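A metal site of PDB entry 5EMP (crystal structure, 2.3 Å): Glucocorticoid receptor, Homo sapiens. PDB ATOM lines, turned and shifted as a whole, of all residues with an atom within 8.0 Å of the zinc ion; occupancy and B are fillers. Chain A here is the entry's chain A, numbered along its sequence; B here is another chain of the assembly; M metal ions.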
ATOM      1  N   LEU A  14     -23.617  -2.351 -14.441  1.00  0.00           N
ATOM      2  CA  LEU A  14     -23.888  -1.635 -15.659  1.00  0.00           C
ATOM      3  C   LEU A  14     -22.862  -0.577 -15.902  1.00  0.00           C
ATOM      4  O   LEU A  14     -22.598   0.212 -15.015  1.00  0.00           O
ATOM      5  CB  LEU A  14     -25.243  -0.976 -15.535  1.00  0.00           C
ATOM      6  CG  LEU A  14     -26.324  -1.715 -16.273  1.00  0.00           C
ATOM      7  CD1 LEU A  14     -26.004  -3.178 -16.427  1.00  0.00           C
ATOM      8  CD2 LEU A  14     -27.670  -1.508 -15.633  1.00  0.00           C
ATOM      9  N   CYS A  15     -22.280  -0.555 -17.091  1.00  0.00           N
ATOM     10  CA  CYS A  15     -21.390   0.549 -17.474  1.00  0.00           C
ATOM     11  C   CYS A  15     -22.076   1.894 -17.330  1.00  0.00           C
ATOM     12  O   CYS A  15     -23.162   2.099 -17.877  1.00  0.00           O
ATOM     13  CB  CYS A  15     -20.944   0.350 -18.922  1.00  0.00           C
ATOM     14  SG  CYS A  15     -19.933   1.664 -19.607  1.00  0.00           S
ATOM     15  N   LEU A  16     -21.455   2.819 -16.608  1.00  0.00           N
ATOM     16  CA  LEU A  16     -22.013   4.155 -16.410  1.00  0.00           C
ATOM     17  C   LEU A  16     -21.971   5.056 -17.643  1.00  0.00           C
ATOM     18  O   LEU A  16     -22.490   6.178 -17.632  1.00  0.00           O
ATOM     19  CB  LEU A  16     -21.305   4.868 -15.262  1.00  0.00           C
ATOM     20  CG  LEU A  16     -21.556   4.250 -13.884  1.00  0.00           C
ATOM     21  CD1 LEU A  16     -20.676   4.896 -12.812  1.00  0.00           C
ATOM     22  CD2 LEU A  16     -23.043   4.368 -13.511  1.00  0.00           C
ATOM     23  N   VAL A  17     -21.343   4.576 -18.718  1.00  0.00           N
ATOM     24  CA  VAL A  17     -21.290   5.353 -19.943  1.00  0.00           C
ATOM     25  C   VAL A  17     -22.333   4.845 -20.930  1.00  0.00           C
ATOM     26  O   VAL A  17     -23.094   5.638 -21.481  1.00  0.00           O
ATOM     27  CB  VAL A  17     -19.882   5.365 -20.577  1.00  0.00           C
ATOM     28  CG1 VAL A  17     -19.913   6.082 -21.934  1.00  0.00           C
ATOM     29  CG2 VAL A  17     -18.890   6.039 -19.641  1.00  0.00           C
ATOM     30  N   CYS A  18     -22.402   3.535 -21.127  1.00  0.00           N
ATOM     31  CA  CYS A  18     -23.276   2.991 -22.163  1.00  0.00           C
ATOM     32  C   CYS A  18     -24.360   2.026 -21.674  1.00  0.00           C
ATOM     33  O   CYS A  18     -25.214   1.602 -22.462  1.00  0.00           O
ATOM     34  CB  CYS A  18     -22.450   2.313 -23.259  1.00  0.00           C
ATOM     35  SG  CYS A  18     -21.832   0.687 -22.823  1.00  0.00           S
ATOM     36  N   SER A  19     -24.314   1.663 -20.389  1.00  0.00           N
ATOM     37  CA  SER A  19     -25.310   0.781 -19.766  1.00  0.00           C
ATOM     38  C   SER A  19     -25.236  -0.689 -20.204  1.00  0.00           C
ATOM     39  O   SER A  19     -26.116  -1.496 -19.859  1.00  0.00           O
ATOM     40  CB  SER A  19     -26.734   1.329 -19.925  1.00  0.00           C
ATOM     41  OG  SER A  19     -26.919   2.470 -19.124  1.00  0.00           O
ATOM     42  N   ASP A  20     -24.201  -1.043 -20.951  1.00  0.00           N
ATOM     43  CA  ASP A  20     -23.869  -2.444 -21.163  1.00  0.00           C
ATOM     44  C   ASP A  20     -23.321  -3.000 -19.846  1.00  0.00           C
ATOM     45  O   ASP A  20     -23.020  -2.238 -18.922  1.00  0.00           O
ATOM     46  CB  ASP A  20     -22.818  -2.584 -22.272  1.00  0.00           C
ATOM     47  CG  ASP A  20     -22.739  -3.993 -22.840  1.00  0.00           C
ATOM     48  OD1 ASP A  20     -23.558  -4.842 -22.436  1.00  0.00           O
ATOM     49  OD2 ASP A  20     -21.865  -4.238 -23.687  1.00  0.00           O
ATOM     50  N   GLU A  21     -23.186  -4.320 -19.759  1.00  0.00           N
ATOM     51  CA  GLU A  21     -22.666  -4.940 -18.540  1.00  0.00           C
ATOM     52  C   GLU A  21     -21.244  -4.463 -18.272  1.00  0.00           C
ATOM     53  O   GLU A  21     -20.357  -4.604 -19.128  1.00  0.00           O
ATOM     54  CB  GLU A  21     -22.668  -6.462 -18.655  1.00  0.00           C
ATOM     55  N   ALA A  22     -21.014  -3.891 -17.092  1.00  0.00           N
ATOM     56  CA  ALA A  22     -19.687  -3.421 -16.742  1.00  0.00           C
ATOM     57  C   ALA A  22     -18.768  -4.611 -16.509  1.00  0.00           C
ATOM     58  O   ALA A  22     -19.230  -5.720 -16.240  1.00  0.00           O
ATOM     59  CB  ALA A  22     -19.740  -2.516 -15.523  1.00  0.00           C
ATOM     60  N   SER A  23     -17.458  -4.386 -16.630  1.00  0.00           N
ATOM     61  CA  SER A  23     -16.493  -5.466 -16.468  1.00  0.00           C
ATOM     62  C   SER A  23     -15.583  -5.244 -15.274  1.00  0.00           C
ATOM     63  O   SER A  23     -14.937  -6.169 -14.793  1.00  0.00           O
ATOM     64  CB  SER A  23     -15.660  -5.625 -17.745  1.00  0.00           C
ATOM     65  OG  SER A  23     -14.776  -4.539 -17.928  1.00  0.00           O
ATOM     66  N   LEU A  30     -16.687   2.775 -13.045  1.00  0.00           N
ATOM     67  CA  LEU A  30     -17.256   1.502 -13.439  1.00  0.00           C
ATOM     68  C   LEU A  30     -17.710   1.533 -14.915  1.00  0.00           C
ATOM     69  O   LEU A  30     -18.713   2.166 -15.247  1.00  0.00           O
ATOM     70  CB  LEU A  30     -18.452   1.188 -12.540  1.00  0.00           C
ATOM     71  CG  LEU A  30     -19.004  -0.226 -12.634  1.00  0.00           C
ATOM     72  CD1 LEU A  30     -17.951  -1.194 -12.151  1.00  0.00           C
ATOM     73  CD2 LEU A  30     -20.295  -0.369 -11.836  1.00  0.00           C
ATOM     74  N   THR A  31     -16.962   0.859 -15.795  1.00  0.00           N
ATOM     75  CA  THR A  31     -17.336   0.806 -17.215  1.00  0.00           C
ATOM     76  C   THR A  31     -17.235  -0.597 -17.810  1.00  0.00           C
ATOM     77  O   THR A  31     -16.745  -1.512 -17.172  1.00  0.00           O
ATOM     78  CB  THR A  31     -16.474   1.746 -18.116  1.00  0.00           C
ATOM     79  OG1 THR A  31     -15.149   1.241 -18.225  1.00  0.00           O
ATOM     80  CG2 THR A  31     -16.452   3.172 -17.598  1.00  0.00           C
ATOM     81  N   CYS A  32     -17.701  -0.728 -19.044  1.00  0.00           N
ATOM     82  CA  CYS A  32     -17.526  -1.948 -19.812  1.00  0.00           C
ATOM     83  C   CYS A  32     -16.147  -1.926 -20.467  1.00  0.00           C
ATOM     84  O   CYS A  32     -15.422  -0.922 -20.391  1.00  0.00           O
ATOM     85  CB  CYS A  32     -18.620  -2.063 -20.877  1.00  0.00           C
ATOM     86  SG  CYS A  32     -18.552  -0.760 -22.125  1.00  0.00           S
ATOM     87  N   GLY A  33     -15.773  -3.026 -21.109  1.00  0.00           N
ATOM     88  CA  GLY A  33     -14.498  -3.129 -21.794  1.00  0.00           C
ATOM     89  C   GLY A  33     -14.385  -2.206 -23.003  1.00  0.00           C
ATOM     90  O   GLY A  33     -13.340  -1.585 -23.219  1.00  0.00           O
ATOM     91  N   SER A  34     -15.453  -2.113 -23.787  1.00  0.00           N
ATOM     92  CA  SER A  34     -15.416  -1.269 -24.985  1.00  0.00           C
ATOM     93  C   SER A  34     -15.246   0.207 -24.601  1.00  0.00           C
ATOM     94  O   SER A  34     -14.461   0.923 -25.228  1.00  0.00           O
ATOM     95  CB  SER A  34     -16.693  -1.462 -25.824  1.00  0.00           C
ATOM     96  OG  SER A  34     -17.819  -1.038 -25.100  1.00  0.00           O
ATOM     97  N   CYS A  35     -15.947   0.638 -23.564  1.00  0.00           N
ATOM     98  CA  CYS A  35     -15.779   2.009 -23.081  1.00  0.00           C
ATOM     99  C   CYS A  35     -14.375   2.320 -22.516  1.00  0.00           C
ATOM    100  O   CYS A  35     -13.860   3.432 -22.706  1.00  0.00           O
ATOM    101  CB  CYS A  35     -16.865   2.374 -22.071  1.00  0.00           C
ATOM    102  SG  CYS A  35     -18.464   2.670 -22.908  1.00  0.00           S
ATOM    103  N   LYS A  36     -13.770   1.355 -21.838  1.00  0.00           N
ATOM    104  CA  LYS A  36     -12.420   1.550 -21.330  1.00  0.00           C
ATOM    105  C   LYS A  36     -11.443   1.865 -22.467  1.00  0.00           C
ATOM    106  O   LYS A  36     -10.722   2.859 -22.412  1.00  0.00           O
ATOM    107  CB  LYS A  36     -11.937   0.319 -20.552  1.00  0.00           C
ATOM    108  CG  LYS A  36     -10.415   0.183 -20.513  1.00  0.00           C
ATOM    109  CD  LYS A  36      -9.998  -1.195 -19.972  1.00  0.00           C
ATOM    110  CE  LYS A  36      -8.695  -1.678 -20.624  1.00  0.00           C
ATOM    111  NZ  LYS A  36      -8.792  -3.081 -21.135  1.00  0.00           N
ATOM    112  N   PHE A  38     -12.156   2.665 -25.623  1.00  0.00           N
ATOM    113  CA  PHE A  38     -12.568   3.856 -26.356  1.00  0.00           C
ATOM    114  C   PHE A  38     -11.999   5.127 -25.687  1.00  0.00           C
ATOM    115  O   PHE A  38     -11.407   5.982 -26.357  1.00  0.00           O
ATOM    116  CB  PHE A  38     -14.094   3.963 -26.472  1.00  0.00           C
ATOM    117  CG  PHE A  38     -14.551   5.268 -27.055  1.00  0.00           C
ATOM    118  CD1 PHE A  38     -14.899   6.335 -26.236  1.00  0.00           C
ATOM    119  CD2 PHE A  38     -14.601   5.446 -28.433  1.00  0.00           C
ATOM    120  CE1 PHE A  38     -15.303   7.549 -26.777  1.00  0.00           C
ATOM    121  CE2 PHE A  38     -15.006   6.647 -28.985  1.00  0.00           C
ATOM    122  CZ  PHE A  38     -15.349   7.712 -28.147  1.00  0.00           C
ATOM    123  N   ILE A  59     -26.383   7.400 -25.479  1.00  0.00           N
ATOM    124  CA  ILE A  59     -25.275   6.469 -25.549  1.00  0.00           C
ATOM    125  C   ILE A  59     -25.676   5.105 -24.981  1.00  0.00           C
ATOM    126  O   ILE A  59     -25.796   4.946 -23.770  1.00  0.00           O
ATOM    127  CB  ILE A  59     -24.059   7.011 -24.791  1.00  0.00           C
ATOM    128  CG1 ILE A  59     -23.674   8.389 -25.331  1.00  0.00           C
ATOM    129  CG2 ILE A  59     -22.876   6.053 -24.921  1.00  0.00           C
ATOM    130  CD1 ILE A  59     -23.262   8.393 -26.830  1.00  0.00           C
ATOM    131  N   ASP A  60     -25.845   4.137 -25.875  1.00  0.00           N
ATOM    132  CA  ASP A  60     -26.354   2.798 -25.587  1.00  0.00           C
ATOM    133  C   ASP A  60     -25.301   1.762 -25.891  1.00  0.00           C
ATOM    134  O   ASP A  60     -24.323   2.063 -26.574  1.00  0.00           O
ATOM    135  CB  ASP A  60     -27.444   2.479 -26.602  1.00  0.00           C
ATOM    136  CG  ASP A  60     -28.792   2.706 -26.064  1.00  0.00           C
ATOM    137  OD1 ASP A  60     -29.708   2.958 -26.869  1.00  0.00           O
ATOM    138  OD2 ASP A  60     -28.918   2.656 -24.822  1.00  0.00           O
ATOM    139  N   LYS A  61     -25.603   0.533 -25.534  1.00  0.00           N
ATOM    140  CA  LYS A  61     -24.923  -0.633 -26.049  1.00  0.00           C
ATOM    141  C   LYS A  61     -24.817  -0.551 -27.545  1.00  0.00           C
ATOM    142  O   LYS A  61     -23.818  -0.885 -28.107  1.00  0.00           O
ATOM    143  CB  LYS A  61     -25.712  -1.884 -25.690  1.00  0.00           C
ATOM    144  CG  LYS A  61     -24.884  -3.139 -25.567  1.00  0.00           C
ATOM    145  CD  LYS A  61     -25.579  -4.373 -26.094  1.00  0.00           C
ATOM    146  CE  LYS A  61     -26.025  -5.295 -24.982  1.00  0.00           C
ATOM    147  NZ  LYS A  61     -26.670  -6.563 -25.425  1.00  0.00           N
ATOM    148  N   ARG A  64     -23.839   3.796 -28.944  1.00  0.00           N
ATOM    149  CA  ARG A  64     -22.517   4.308 -28.597  1.00  0.00           C
ATOM    150  C   ARG A  64     -21.545   4.381 -29.752  1.00  0.00           C
ATOM    151  O   ARG A  64     -20.619   5.120 -29.719  1.00  0.00           O
ATOM    152  CB  ARG A  64     -21.927   3.554 -27.401  1.00  0.00           C
ATOM    153  CG  ARG A  64     -21.131   2.322 -27.752  1.00  0.00           C
ATOM    154  CD  ARG A  64     -21.098   1.270 -26.685  1.00  0.00           C
ATOM    155  NE  ARG A  64     -20.569   0.020 -27.198  1.00  0.00           N
ATOM    156  CZ  ARG A  64     -20.609  -1.137 -26.551  1.00  0.00           C
ATOM    157  NH1 ARG A  64     -20.111  -2.200 -27.108  1.00  0.00           N
ATOM    158  NH2 ARG A  64     -21.099  -1.220 -25.348  1.00  0.00           N
ATOM    159  N   ARG A  71     -20.045  10.199 -26.801  1.00  0.00           N
ATOM    160  CA  ARG A  71     -19.546   9.128 -25.948  1.00  0.00           C
ATOM    161  C   ARG A  71     -18.339   9.607 -25.124  1.00  0.00           C
ATOM    162  O   ARG A  71     -18.259   9.350 -23.928  1.00  0.00           O
ATOM    163  CB  ARG A  71     -19.188   7.911 -26.774  1.00  0.00           C
ATOM    164  CG  ARG A  71     -18.814   6.665 -25.996  1.00  0.00           C
ATOM    165  CD  ARG A  71     -18.349   5.554 -26.965  1.00  0.00           C
ATOM    166  NE  ARG A  71     -18.171   4.264 -26.292  1.00  0.00           N
ATOM    167  CZ  ARG A  71     -17.758   3.150 -26.884  1.00  0.00           C
ATOM    168  NH1 ARG A  71     -17.464   3.164 -28.175  1.00  0.00           N
ATOM    169  NH2 ARG A  71     -17.639   2.037 -26.184  1.00  0.00           N
ATOM    170  N   CYS A  75     -17.990  10.130 -21.165  1.00  0.00           N
ATOM    171  CA  CYS A  75     -16.897   9.538 -20.409  1.00  0.00           C
ATOM    172  C   CYS A  75     -16.320  10.523 -19.407  1.00  0.00           C
ATOM    173  O   CYS A  75     -16.112  10.173 -18.247  1.00  0.00           O
ATOM    174  CB  CYS A  75     -15.778   9.051 -21.332  1.00  0.00           C
ATOM    175  SG  CYS A  75     -16.124   7.497 -22.172  1.00  0.00           S
ATOM    176  N   MET A  80     -14.138   9.653 -15.782  1.00  0.00           N
ATOM    177  CA  MET A  80     -13.024   8.882 -16.315  1.00  0.00           C
ATOM    178  C   MET A  80     -11.780   9.749 -16.457  1.00  0.00           C
ATOM    179  O   MET A  80     -11.869  10.935 -16.773  1.00  0.00           O
ATOM    180  CB  MET A  80     -13.395   8.218 -17.636  1.00  0.00           C
ATOM    181  CG  MET A  80     -14.575   7.260 -17.519  1.00  0.00           C
ATOM    182  SD  MET A  80     -14.831   6.309 -19.031  1.00  0.00           S
ATOM    183  CE  MET A  80     -13.287   5.368 -19.038  1.00  0.00           C
ATOM    184  P    DG B  13     -17.830  -0.490 -29.593  1.00  0.00           P
ATOM    185  OP1  DG B  13     -19.308  -0.615 -29.572  1.00  0.00           O
ATOM    186  OP2  DG B  13     -17.191   0.477 -28.667  1.00  0.00           O
ATOM    187  O5'  DG B  13     -17.237  -1.949 -29.397  1.00  0.00           O
ATOM    188  C5'  DG B  13     -17.637  -2.977 -30.292  1.00  0.00           C
ATOM    189  C4'  DG B  13     -16.981  -4.302 -29.902  1.00  0.00           C
ATOM    190  O4'  DG B  13     -15.635  -4.335 -30.439  1.00  0.00           O
ATOM    191  C3'  DG B  13     -16.849  -4.562 -28.405  1.00  0.00           C
ATOM    192  O3'  DG B  13     -17.181  -5.918 -28.155  1.00  0.00           O
ATOM    193  C2'  DG B  13     -15.391  -4.264 -28.094  1.00  0.00           C
ATOM    194  C1'  DG B  13     -14.741  -4.691 -29.400  1.00  0.00           C
ATOM    195  N9   DG B  13     -13.457  -4.059 -29.658  1.00  0.00           N
ATOM    196  C8   DG B  13     -13.115  -2.730 -29.534  1.00  0.00           C
ATOM    197  N7   DG B  13     -11.877  -2.478 -29.861  1.00  0.00           N
ATOM    198  C5   DG B  13     -11.371  -3.734 -30.199  1.00  0.00           C
ATOM    199  C6   DG B  13     -10.085  -4.118 -30.616  1.00  0.00           C
ATOM    200  O6   DG B  13      -9.094  -3.384 -30.764  1.00  0.00           O
ATOM    201  N1   DG B  13     -10.011  -5.495 -30.859  1.00  0.00           N
ATOM    202  C2   DG B  13     -11.063  -6.386 -30.707  1.00  0.00           C
ATOM    203  N2   DG B  13     -10.836  -7.669 -30.972  1.00  0.00           N
ATOM    204  N3   DG B  13     -12.268  -6.029 -30.309  1.00  0.00           N
ATOM    205  C4   DG B  13     -12.339  -4.707 -30.077  1.00  0.00           C
HETATM  206 ZN    ZN M   1     -19.794   1.146 -21.808  1.00  0.00          ZN
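The backbone NH (N) of Cys 15 sits at hydrogen-bond distance from the backbone carbonyl oxygen (O) of Asp 20, 2.6 Å away.
The side-chain sulfur of Cys 18 sits close to the backbone NH of Asp 20.
The backbone carbonyl oxygen (O) of Cys 18 sits at hydrogen-bond distance from the backbone NH (N) of Lys 61.
The side-chain sulfur (SG) of Cys 18 lies close to the guanidinium group (NH2) of Arg 64 (3.2 Å).
OG of Ser 34 sits close to SG of Cys 32, 3.1 Å away.
SG of Cys 35 lies close to NH2 of Arg 71 (3.4 Å).
N of Val 17 sits close to SG of Cys 15, 3.4 Å away.
The zinc ion is bound by SG of Cys 15 (2.3 Å), SG of Cys 32 (2.3 Å), SG of Cys 35 (2.3 Å) and SG of Cys 18 (2.3 Å).
The zinc ion has four donor atoms within binding distance.
Of the 26 residues printed, 4 come within 4 Å of the zinc ion.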
